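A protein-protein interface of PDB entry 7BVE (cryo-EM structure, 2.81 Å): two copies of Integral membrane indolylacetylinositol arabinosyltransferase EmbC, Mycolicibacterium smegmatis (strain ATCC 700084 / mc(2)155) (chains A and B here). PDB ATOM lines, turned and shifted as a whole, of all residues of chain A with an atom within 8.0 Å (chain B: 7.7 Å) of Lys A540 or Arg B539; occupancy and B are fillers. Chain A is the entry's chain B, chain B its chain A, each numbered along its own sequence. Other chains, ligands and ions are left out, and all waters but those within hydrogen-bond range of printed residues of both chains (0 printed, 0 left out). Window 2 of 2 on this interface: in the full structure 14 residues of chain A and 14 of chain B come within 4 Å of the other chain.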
ATOM      1  N   ILE A 534      -0.040  -5.348  19.985  1.00  0.00           N
ATOM      2  CA  ILE A 534       1.222  -4.605  19.929  1.00  0.00           C
ATOM      3  C   ILE A 534       1.037  -3.262  19.230  1.00  0.00           C
ATOM      4  O   ILE A 534       1.580  -2.241  19.671  1.00  0.00           O
ATOM      5  CB  ILE A 534       2.311  -5.458  19.248  1.00  0.00           C
ATOM      6  CG1 ILE A 534       2.700  -6.639  20.123  1.00  0.00           C
ATOM      7  CG2 ILE A 534       3.552  -4.655  18.946  1.00  0.00           C
ATOM      8  CD1 ILE A 534       3.592  -7.617  19.425  1.00  0.00           C
ATOM      9  N   ALA A 535       0.235  -3.227  18.160  1.00  0.00           N
ATOM     10  CA  ALA A 535       0.029  -1.980  17.430  1.00  0.00           C
ATOM     11  C   ALA A 535      -0.761  -0.967  18.247  1.00  0.00           C
ATOM     12  O   ALA A 535      -0.478   0.233  18.191  1.00  0.00           O
ATOM     13  CB  ALA A 535      -0.678  -2.257  16.110  1.00  0.00           C
ATOM     14  N   MET A 536      -1.742  -1.426  19.025  1.00  0.00           N
ATOM     15  CA  MET A 536      -2.490  -0.495  19.860  1.00  0.00           C
ATOM     16  C   MET A 536      -1.685  -0.059  21.080  1.00  0.00           C
ATOM     17  O   MET A 536      -1.888   1.045  21.590  1.00  0.00           O
ATOM     18  CB  MET A 536      -3.816  -1.130  20.264  1.00  0.00           C
ATOM     19  CG  MET A 536      -4.792  -0.209  20.962  1.00  0.00           C
ATOM     20  SD  MET A 536      -5.259   1.186  19.939  1.00  0.00           S
ATOM     21  CE  MET A 536      -6.222   0.358  18.690  1.00  0.00           C
ATOM     22  N   THR A 537      -0.756  -0.893  21.552  1.00  0.00           N
ATOM     23  CA  THR A 537       0.131  -0.466  22.629  1.00  0.00           C
ATOM     24  C   THR A 537       1.166   0.545  22.145  1.00  0.00           C
ATOM     25  O   THR A 537       1.517   1.470  22.885  1.00  0.00           O
ATOM     26  CB  THR A 537       0.809  -1.691  23.243  1.00  0.00           C
ATOM     27  OG1 THR A 537      -0.196  -2.622  23.650  1.00  0.00           O
ATOM     28  CG2 THR A 537       1.615  -1.329  24.464  1.00  0.00           C
ATOM     29  N   LEU A 538       1.647   0.411  20.907  1.00  0.00           N
ATOM     30  CA  LEU A 538       2.576   1.400  20.366  1.00  0.00           C
ATOM     31  C   LEU A 538       1.879   2.712  20.044  1.00  0.00           C
ATOM     32  O   LEU A 538       2.390   3.783  20.380  1.00  0.00           O
ATOM     33  CB  LEU A 538       3.269   0.873  19.115  1.00  0.00           C
ATOM     34  CG  LEU A 538       4.347  -0.190  19.247  1.00  0.00           C
ATOM     35  CD1 LEU A 538       4.797  -0.609  17.878  1.00  0.00           C
ATOM     36  CD2 LEU A 538       5.502   0.358  20.034  1.00  0.00           C
ATOM     37  N   ARG A 539       0.718   2.644  19.381  1.00  0.00           N
ATOM     38  CA  ARG A 539       0.061   3.833  18.840  1.00  0.00           C
ATOM     39  C   ARG A 539      -0.370   4.788  19.942  1.00  0.00           C
ATOM     40  O   ARG A 539       0.095   5.928  20.010  1.00  0.00           O
ATOM     41  CB  ARG A 539      -1.145   3.424  18.002  1.00  0.00           C
ATOM     42  CG  ARG A 539      -1.888   4.595  17.426  1.00  0.00           C
ATOM     43  CD  ARG A 539      -1.039   5.280  16.400  1.00  0.00           C
ATOM     44  NE  ARG A 539      -1.701   6.427  15.799  1.00  0.00           N
ATOM     45  CZ  ARG A 539      -1.106   7.257  14.953  1.00  0.00           C
ATOM     46  NH1 ARG A 539       0.153   7.052  14.606  1.00  0.00           N
ATOM     47  NH2 ARG A 539      -1.767   8.285  14.446  1.00  0.00           N
ATOM     48  N   LYS A 540      -1.246   4.336  20.820  1.00  0.00           N
ATOM     49  CA  LYS A 540      -1.581   5.092  22.009  1.00  0.00           C
ATOM     50  C   LYS A 540      -0.556   4.789  23.091  1.00  0.00           C
ATOM     51  O   LYS A 540       0.457   4.138  22.848  1.00  0.00           O
ATOM     52  CB  LYS A 540      -2.997   4.755  22.452  1.00  0.00           C
ATOM     53  CG  LYS A 540      -4.010   5.135  21.395  1.00  0.00           C
ATOM     54  CD  LYS A 540      -5.417   4.798  21.788  1.00  0.00           C
ATOM     55  CE  LYS A 540      -6.394   5.331  20.757  1.00  0.00           C
ATOM     56  NZ  LYS A 540      -6.233   4.654  19.450  1.00  0.00           N
ATOM     57  N   GLY A 541      -0.801   5.287  24.295  1.00  0.00           N
ATOM     58  CA  GLY A 541       0.063   4.904  25.396  1.00  0.00           C
ATOM     59  C   GLY A 541      -0.157   3.462  25.798  1.00  0.00           C
ATOM     60  O   GLY A 541       0.787   2.747  26.142  1.00  0.00           O
ATOM     61  N   ARG A 542      -1.401   3.010  25.719  1.00  0.00           N
ATOM     62  CA  ARG A 542      -1.838   1.698  26.154  1.00  0.00           C
ATOM     63  C   ARG A 542      -3.221   1.466  25.568  1.00  0.00           C
ATOM     64  O   ARG A 542      -3.826   2.377  24.998  1.00  0.00           O
ATOM     65  CB  ARG A 542      -1.891   1.615  27.672  1.00  0.00           C
ATOM     66  CG  ARG A 542      -2.931   2.540  28.227  1.00  0.00           C
ATOM     67  CD  ARG A 542      -2.965   2.513  29.721  1.00  0.00           C
ATOM     68  NE  ARG A 542      -4.072   3.316  30.212  1.00  0.00           N
ATOM     69  CZ  ARG A 542      -4.363   3.476  31.494  1.00  0.00           C
ATOM     70  NH1 ARG A 542      -3.616   2.892  32.419  1.00  0.00           N
ATOM     71  NH2 ARG A 542      -5.397   4.224  31.849  1.00  0.00           N
ATOM     72  N   ILE A 543      -3.712   0.242  25.711  1.00  0.00           N
ATOM     73  CA  ILE A 543      -5.114  -0.018  25.370  1.00  0.00           C
ATOM     74  C   ILE A 543      -5.992   0.691  26.394  1.00  0.00           C
ATOM     75  O   ILE A 543      -5.822   0.460  27.603  1.00  0.00           O
ATOM     76  CB  ILE A 543      -5.376  -1.530  25.346  1.00  0.00           C
ATOM     77  CG1 ILE A 543      -4.457  -2.189  24.323  1.00  0.00           C
ATOM     78  CG2 ILE A 543      -6.804  -1.832  24.996  1.00  0.00           C
ATOM     79  CD1 ILE A 543      -4.385  -3.671  24.440  1.00  0.00           C
ATOM     80  N   PRO A 544      -6.936   1.568  25.970  1.00  0.00           N
ATOM     81  CA  PRO A 544      -7.434   2.650  26.841  1.00  0.00           C
ATOM     82  C   PRO A 544      -8.121   2.278  28.147  1.00  0.00           C
ATOM     83  O   PRO A 544      -7.824   2.881  29.183  1.00  0.00           O
ATOM     84  CB  PRO A 544      -8.418   3.388  25.928  1.00  0.00           C
ATOM     85  CG  PRO A 544      -7.923   3.134  24.575  1.00  0.00           C
ATOM     86  CD  PRO A 544      -7.411   1.739  24.587  1.00  0.00           C
ATOM     87  N   ARG A 552       1.024  -4.998  29.660  1.00  0.00           N
ATOM     88  CA  ARG A 552       2.433  -5.075  29.283  1.00  0.00           C
ATOM     89  C   ARG A 552       3.008  -6.462  29.530  1.00  0.00           C
ATOM     90  O   ARG A 552       3.723  -7.013  28.683  1.00  0.00           O
ATOM     91  CB  ARG A 552       3.247  -4.052  30.069  1.00  0.00           C
ATOM     92  CG  ARG A 552       3.012  -2.600  29.747  1.00  0.00           C
ATOM     93  CD  ARG A 552       3.974  -1.762  30.577  1.00  0.00           C
ATOM     94  NE  ARG A 552       3.745  -0.331  30.446  1.00  0.00           N
ATOM     95  CZ  ARG A 552       4.285   0.423  29.497  1.00  0.00           C
ATOM     96  NH1 ARG A 552       5.079  -0.123  28.588  1.00  0.00           N
ATOM     97  NH2 ARG A 552       4.023   1.720  29.455  1.00  0.00           N
ATOM     98  N   ALA A 593      -9.168  -3.881  22.277  1.00  0.00           N
ATOM     99  CA  ALA A 593      -8.411  -3.021  21.375  1.00  0.00           C
ATOM    100  C   ALA A 593      -9.109  -2.738  20.051  1.00  0.00           C
ATOM    101  O   ALA A 593      -8.529  -2.048  19.213  1.00  0.00           O
ATOM    102  CB  ALA A 593      -7.046  -3.644  21.091  1.00  0.00           C
ATOM    103  N   THR A 597     -14.897   2.464  21.428  1.00  0.00           N
ATOM    104  CA  THR A 597     -14.237   3.265  22.450  1.00  0.00           C
ATOM    105  C   THR A 597     -12.732   3.364  22.215  1.00  0.00           C
ATOM    106  O   THR A 597     -12.142   4.426  22.439  1.00  0.00           O
ATOM    107  CB  THR A 597     -14.528   2.661  23.826  1.00  0.00           C
ATOM    108  OG1 THR A 597     -15.943   2.506  23.979  1.00  0.00           O
ATOM    109  CG2 THR A 597     -14.023   3.559  24.945  1.00  0.00           C
ATOM    110  N   ALA A 598     -12.102   2.293  21.736  1.00  0.00           N
ATOM    111  CA  ALA A 598     -10.657   2.279  21.549  1.00  0.00           C
ATOM    112  C   ALA A 598     -10.243   2.691  20.143  1.00  0.00           C
ATOM    113  O   ALA A 598      -9.380   3.556  19.979  1.00  0.00           O
ATOM    114  CB  ALA A 598     -10.103   0.891  21.869  1.00  0.00           C
ATOM    115  N   MET A 599     -10.831   2.081  19.124  1.00  0.00           N
ATOM    116  CA  MET A 599     -10.473   2.339  17.731  1.00  0.00           C
ATOM    117  C   MET A 599     -11.607   3.141  17.108  1.00  0.00           C
ATOM    118  O   MET A 599     -12.676   2.603  16.820  1.00  0.00           O
ATOM    119  CB  MET A 599     -10.220   1.029  16.999  1.00  0.00           C
ATOM    120  CG  MET A 599      -9.684   1.182  15.610  1.00  0.00           C
ATOM    121  SD  MET A 599      -9.401  -0.409  14.822  1.00  0.00           S
ATOM    122  CE  MET A 599      -7.905  -0.938  15.625  1.00  0.00           C
ATOM    123  N   LYS A 600     -11.361   4.430  16.882  1.00  0.00           N
ATOM    124  CA  LYS A 600     -12.411   5.407  16.634  1.00  0.00           C
ATOM    125  C   LYS A 600     -12.872   5.489  15.185  1.00  0.00           C
ATOM    126  O   LYS A 600     -13.981   5.971  14.942  1.00  0.00           O
ATOM    127  CB  LYS A 600     -11.938   6.795  17.062  1.00  0.00           C
ATOM    128  CG  LYS A 600     -11.644   6.949  18.538  1.00  0.00           C
ATOM    129  CD  LYS A 600     -12.916   6.935  19.356  1.00  0.00           C
ATOM    130  CE  LYS A 600     -12.631   7.275  20.805  1.00  0.00           C
ATOM    131  NZ  LYS A 600     -13.868   7.259  21.628  1.00  0.00           N
ATOM    132  N   SER A 601     -12.067   5.064  14.221  1.00  0.00           N
ATOM    133  CA  SER A 601     -12.399   5.219  12.813  1.00  0.00           C
ATOM    134  C   SER A 601     -12.867   3.892  12.245  1.00  0.00           C
ATOM    135  O   SER A 601     -12.220   2.864  12.456  1.00  0.00           O
ATOM    136  CB  SER A 601     -11.199   5.709  12.016  1.00  0.00           C
ATOM    137  OG  SER A 601     -10.236   4.685  11.935  1.00  0.00           O
ATOM    138  N   ASN A 604     -10.487   1.756   9.925  1.00  0.00           N
ATOM    139  CA  ASN A 604      -9.568   0.817  10.556  1.00  0.00           C
ATOM    140  C   ASN A 604     -10.279  -0.457  10.988  1.00  0.00           C
ATOM    141  O   ASN A 604      -9.718  -1.555  10.893  1.00  0.00           O
ATOM    142  CB  ASN A 604      -8.904   1.480  11.756  1.00  0.00           C
ATOM    143  CG  ASN A 604      -7.980   2.597  11.365  1.00  0.00           C
ATOM    144  OD1 ASN A 604      -7.256   2.506  10.384  1.00  0.00           O
ATOM    145  ND2 ASN A 604      -7.987   3.660  12.145  1.00  0.00           N
ATOM    146  N   SER B 533      10.760   1.015  10.827  1.00  0.00           N
ATOM    147  CA  SER B 533      10.086   2.192  10.287  1.00  0.00           C
ATOM    148  C   SER B 533       8.602   2.212  10.647  1.00  0.00           C
ATOM    149  O   SER B 533       8.063   3.267  11.007  1.00  0.00           O
ATOM    150  CB  SER B 533      10.270   2.235   8.779  1.00  0.00           C
ATOM    151  OG  SER B 533      11.641   2.304   8.453  1.00  0.00           O
ATOM    152  N   ILE B 534       7.934   1.052  10.590  1.00  0.00           N
ATOM    153  CA  ILE B 534       6.521   0.972  10.969  1.00  0.00           C
ATOM    154  C   ILE B 534       6.335   1.253  12.458  1.00  0.00           C
ATOM    155  O   ILE B 534       5.399   1.958  12.856  1.00  0.00           O
ATOM    156  CB  ILE B 534       5.940  -0.398  10.570  1.00  0.00           C
ATOM    157  CG1 ILE B 534       5.848  -0.529   9.058  1.00  0.00           C
ATOM    158  CG2 ILE B 534       4.569  -0.626  11.155  1.00  0.00           C
ATOM    159  CD1 ILE B 534       5.499  -1.912   8.609  1.00  0.00           C
ATOM    160  N   ALA B 535       7.240   0.743  13.300  1.00  0.00           N
ATOM    161  CA  ALA B 535       7.114   0.952  14.739  1.00  0.00           C
ATOM    162  C   ALA B 535       7.342   2.407  15.124  1.00  0.00           C
ATOM    163  O   ALA B 535       6.668   2.926  16.019  1.00  0.00           O
ATOM    164  CB  ALA B 535       8.087   0.052  15.487  1.00  0.00           C
ATOM    165  N   MET B 536       8.271   3.089  14.454  1.00  0.00           N
ATOM    166  CA  MET B 536       8.486   4.499  14.759  1.00  0.00           C
ATOM    167  C   MET B 536       7.381   5.375  14.179  1.00  0.00           C
ATOM    168  O   MET B 536       7.088   6.440  14.728  1.00  0.00           O
ATOM    169  CB  MET B 536       9.860   4.923  14.252  1.00  0.00           C
ATOM    170  CG  MET B 536      10.309   6.304  14.674  1.00  0.00           C
ATOM    171  SD  MET B 536      10.420   6.470  16.454  1.00  0.00           S
ATOM    172  CE  MET B 536      11.813   5.412  16.789  1.00  0.00           C
ATOM    173  N   THR B 537       6.740   4.944  13.092  1.00  0.00           N
ATOM    174  CA  THR B 537       5.588   5.680  12.580  1.00  0.00           C
ATOM    175  C   THR B 537       4.363   5.505  13.472  1.00  0.00           C
ATOM    176  O   THR B 537       3.587   6.450  13.644  1.00  0.00           O
ATOM    177  CB  THR B 537       5.291   5.228  11.150  1.00  0.00           C
ATOM    178  OG1 THR B 537       6.474   5.378  10.362  1.00  0.00           O
ATOM    179  CG2 THR B 537       4.211   6.065  10.515  1.00  0.00           C
ATOM    180  N   LEU B 538       4.183   4.325  14.070  1.00  0.00           N
ATOM    181  CA  LEU B 538       3.071   4.131  15.000  1.00  0.00           C
ATOM    182  C   LEU B 538       3.304   4.857  16.315  1.00  0.00           C
ATOM    183  O   LEU B 538       2.397   5.522  16.824  1.00  0.00           O
ATOM    184  CB  LEU B 538       2.836   2.649  15.271  1.00  0.00           C
ATOM    185  CG  LEU B 538       2.202   1.783  14.197  1.00  0.00           C
ATOM    186  CD1 LEU B 538       2.172   0.358  14.666  1.00  0.00           C
ATOM    187  CD2 LEU B 538       0.810   2.270  13.912  1.00  0.00           C
ATOM    188  N   ARG B 539       4.508   4.727  16.884  1.00  0.00           N
ATOM    189  CA  ARG B 539       4.784   5.205  18.239  1.00  0.00           C
ATOM    190  C   ARG B 539       4.654   6.716  18.341  1.00  0.00           C
ATOM    191  O   ARG B 539       3.809   7.232  19.077  1.00  0.00           O
ATOM    192  CB  ARG B 539       6.181   4.772  18.667  1.00  0.00           C
ATOM    193  CG  ARG B 539       6.548   5.244  20.046  1.00  0.00           C
ATOM    194  CD  ARG B 539       5.700   4.545  21.065  1.00  0.00           C
ATOM    195  NE  ARG B 539       6.005   4.956  22.426  1.00  0.00           N
ATOM    196  CZ  ARG B 539       5.309   4.561  23.484  1.00  0.00           C
ATOM    197  NH1 ARG B 539       4.285   3.741  23.329  1.00  0.00           N
ATOM    198  NH2 ARG B 539       5.640   4.978  24.696  1.00  0.00           N
ATOM    199  N   LYS B 540       5.469   7.440  17.596  1.00  0.00           N
ATOM    200  CA  LYS B 540       5.305   8.875  17.476  1.00  0.00           C
ATOM    201  C   LYS B 540       4.283   9.161  16.387  1.00  0.00           C
ATOM    202  O   LYS B 540       3.624   8.261  15.874  1.00  0.00           O
ATOM    203  CB  LYS B 540       6.650   9.525  17.185  1.00  0.00           C
ATOM    204  CG  LYS B 540       7.630   9.294  18.315  1.00  0.00           C
ATOM    205  CD  LYS B 540       8.975   9.905  18.056  1.00  0.00           C
ATOM    206  CE  LYS B 540       9.863   9.765  19.278  1.00  0.00           C
ATOM    207  NZ  LYS B 540      10.184   8.347  19.562  1.00  0.00           N
ATOM    208  N   GLY B 541       4.124  10.432  16.044  1.00  0.00           N
ATOM    209  CA  GLY B 541       3.272  10.747  14.913  1.00  0.00           C
ATOM    210  C   GLY B 541       3.911  10.334  13.605  1.00  0.00           C
ATOM    211  O   GLY B 541       3.234   9.864  12.689  1.00  0.00           O
ATOM    212  N   ARG B 542       5.228  10.464  13.526  1.00  0.00           N
ATOM    213  CA  ARG B 542       6.018  10.222  12.332  1.00  0.00           C
ATOM    214  C   ARG B 542       7.472  10.144  12.763  1.00  0.00           C
ATOM    215  O   ARG B 542       7.805  10.429  13.916  1.00  0.00           O
ATOM    216  CB  ARG B 542       5.829  11.339  11.318  1.00  0.00           C
ATOM    217  CG  ARG B 542       6.367  12.636  11.841  1.00  0.00           C
ATOM    218  CD  ARG B 542       6.151  13.762  10.885  1.00  0.00           C
ATOM    219  NE  ARG B 542       6.811  14.961  11.370  1.00  0.00           N
ATOM    220  CZ  ARG B 542       6.808  16.122  10.731  1.00  0.00           C
ATOM    221  NH1 ARG B 542       6.163  16.242   9.581  1.00  0.00           N
ATOM    222  NH2 ARG B 542       7.445  17.162  11.248  1.00  0.00           N
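Of the 19 printed residues of chain A, 4 touch a printed residue of chain B. Printed residues of chain A that touch a printed residue of chain B: Thr A537, Leu A538, Arg A539 and Lys A540. Along chain B the printed residues that touch a printed residue of chain A span positions 537 to 540. Among the printed residues, 7 pairs touch across the chains. Among the printed residues, no Asp or Glu carboxylate lies within 4 Å of a Lys or Arg side-chain nitrogen of the other chain.
Thr A537 touches Arg B539, and with the chains exchanged Arg A539 touches Thr B537. Leu A538 touches its own counterpart, Leu B538. Leu A538 touches Arg B539, and with the chains exchanged Arg A539 touches Leu B538. Arg A539 touches Lys B540, and with the chains exchanged Lys A540 touches Arg B539. Positions printed for both chains: 534, 535, 536, 537, 538, 539, 540, 541 and 542. Of the 7 pairs that touch across the chains among the printed residues, 7 have their exchanged pair printed and touching as well.
Of the printed residues of chain A, Arg B539 touches Thr A537, Leu A538 and Lys A540. Printed residues of chain B within 4 Å of Thr A537: Arg B539 (3.6 Å). Printed residues of chain A within 4 Å of Lys B540: Arg A539. Of the printed residues of chain B, Arg A539 touches Thr B537, Leu B538 and Lys B540. Printed residues of chain A within 4 Å of Thr B537: Arg A539. Asn A604 touches none of the printed residues of chain B. Thr A597 touches none of the printed residues of chain B.
The backbone carbonyl oxygen of Ser B533 sits at hydrogen-bond distance from the side-chain hydroxyl of Thr B537, 2.7 Å away. The side-chain sulfur (SD) of Met B536 sits at hydrogen-bond distance from the side-chain amino group (NZ) of Lys B540, 3.6 Å away. The side-chain sulfur of Met A536 sits at hydrogen-bond distance from the side-chain amino group of Lys A540, at 3.6 Å. The backbone carbonyl oxygen of Ala A598 sits at hydrogen-bond distance from the side-chain amino group of Lys A540, 3.4 Å away.
Arg B539 touches Thr A537 (NH1 to O, 3.6 Å). O of Leu B538 touches O of Leu A538, at 3.96 Å. Arg B539 touches Leu A538 (CD to O, 3.5 Å). Thr B537 touches Arg A539. CD of Arg A539 touches O of Leu B538, at 3.5 Å. Arg A539 touches Lys B540. O of Lys A540 touches NH1 of Arg B539, at 3.9 Å.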
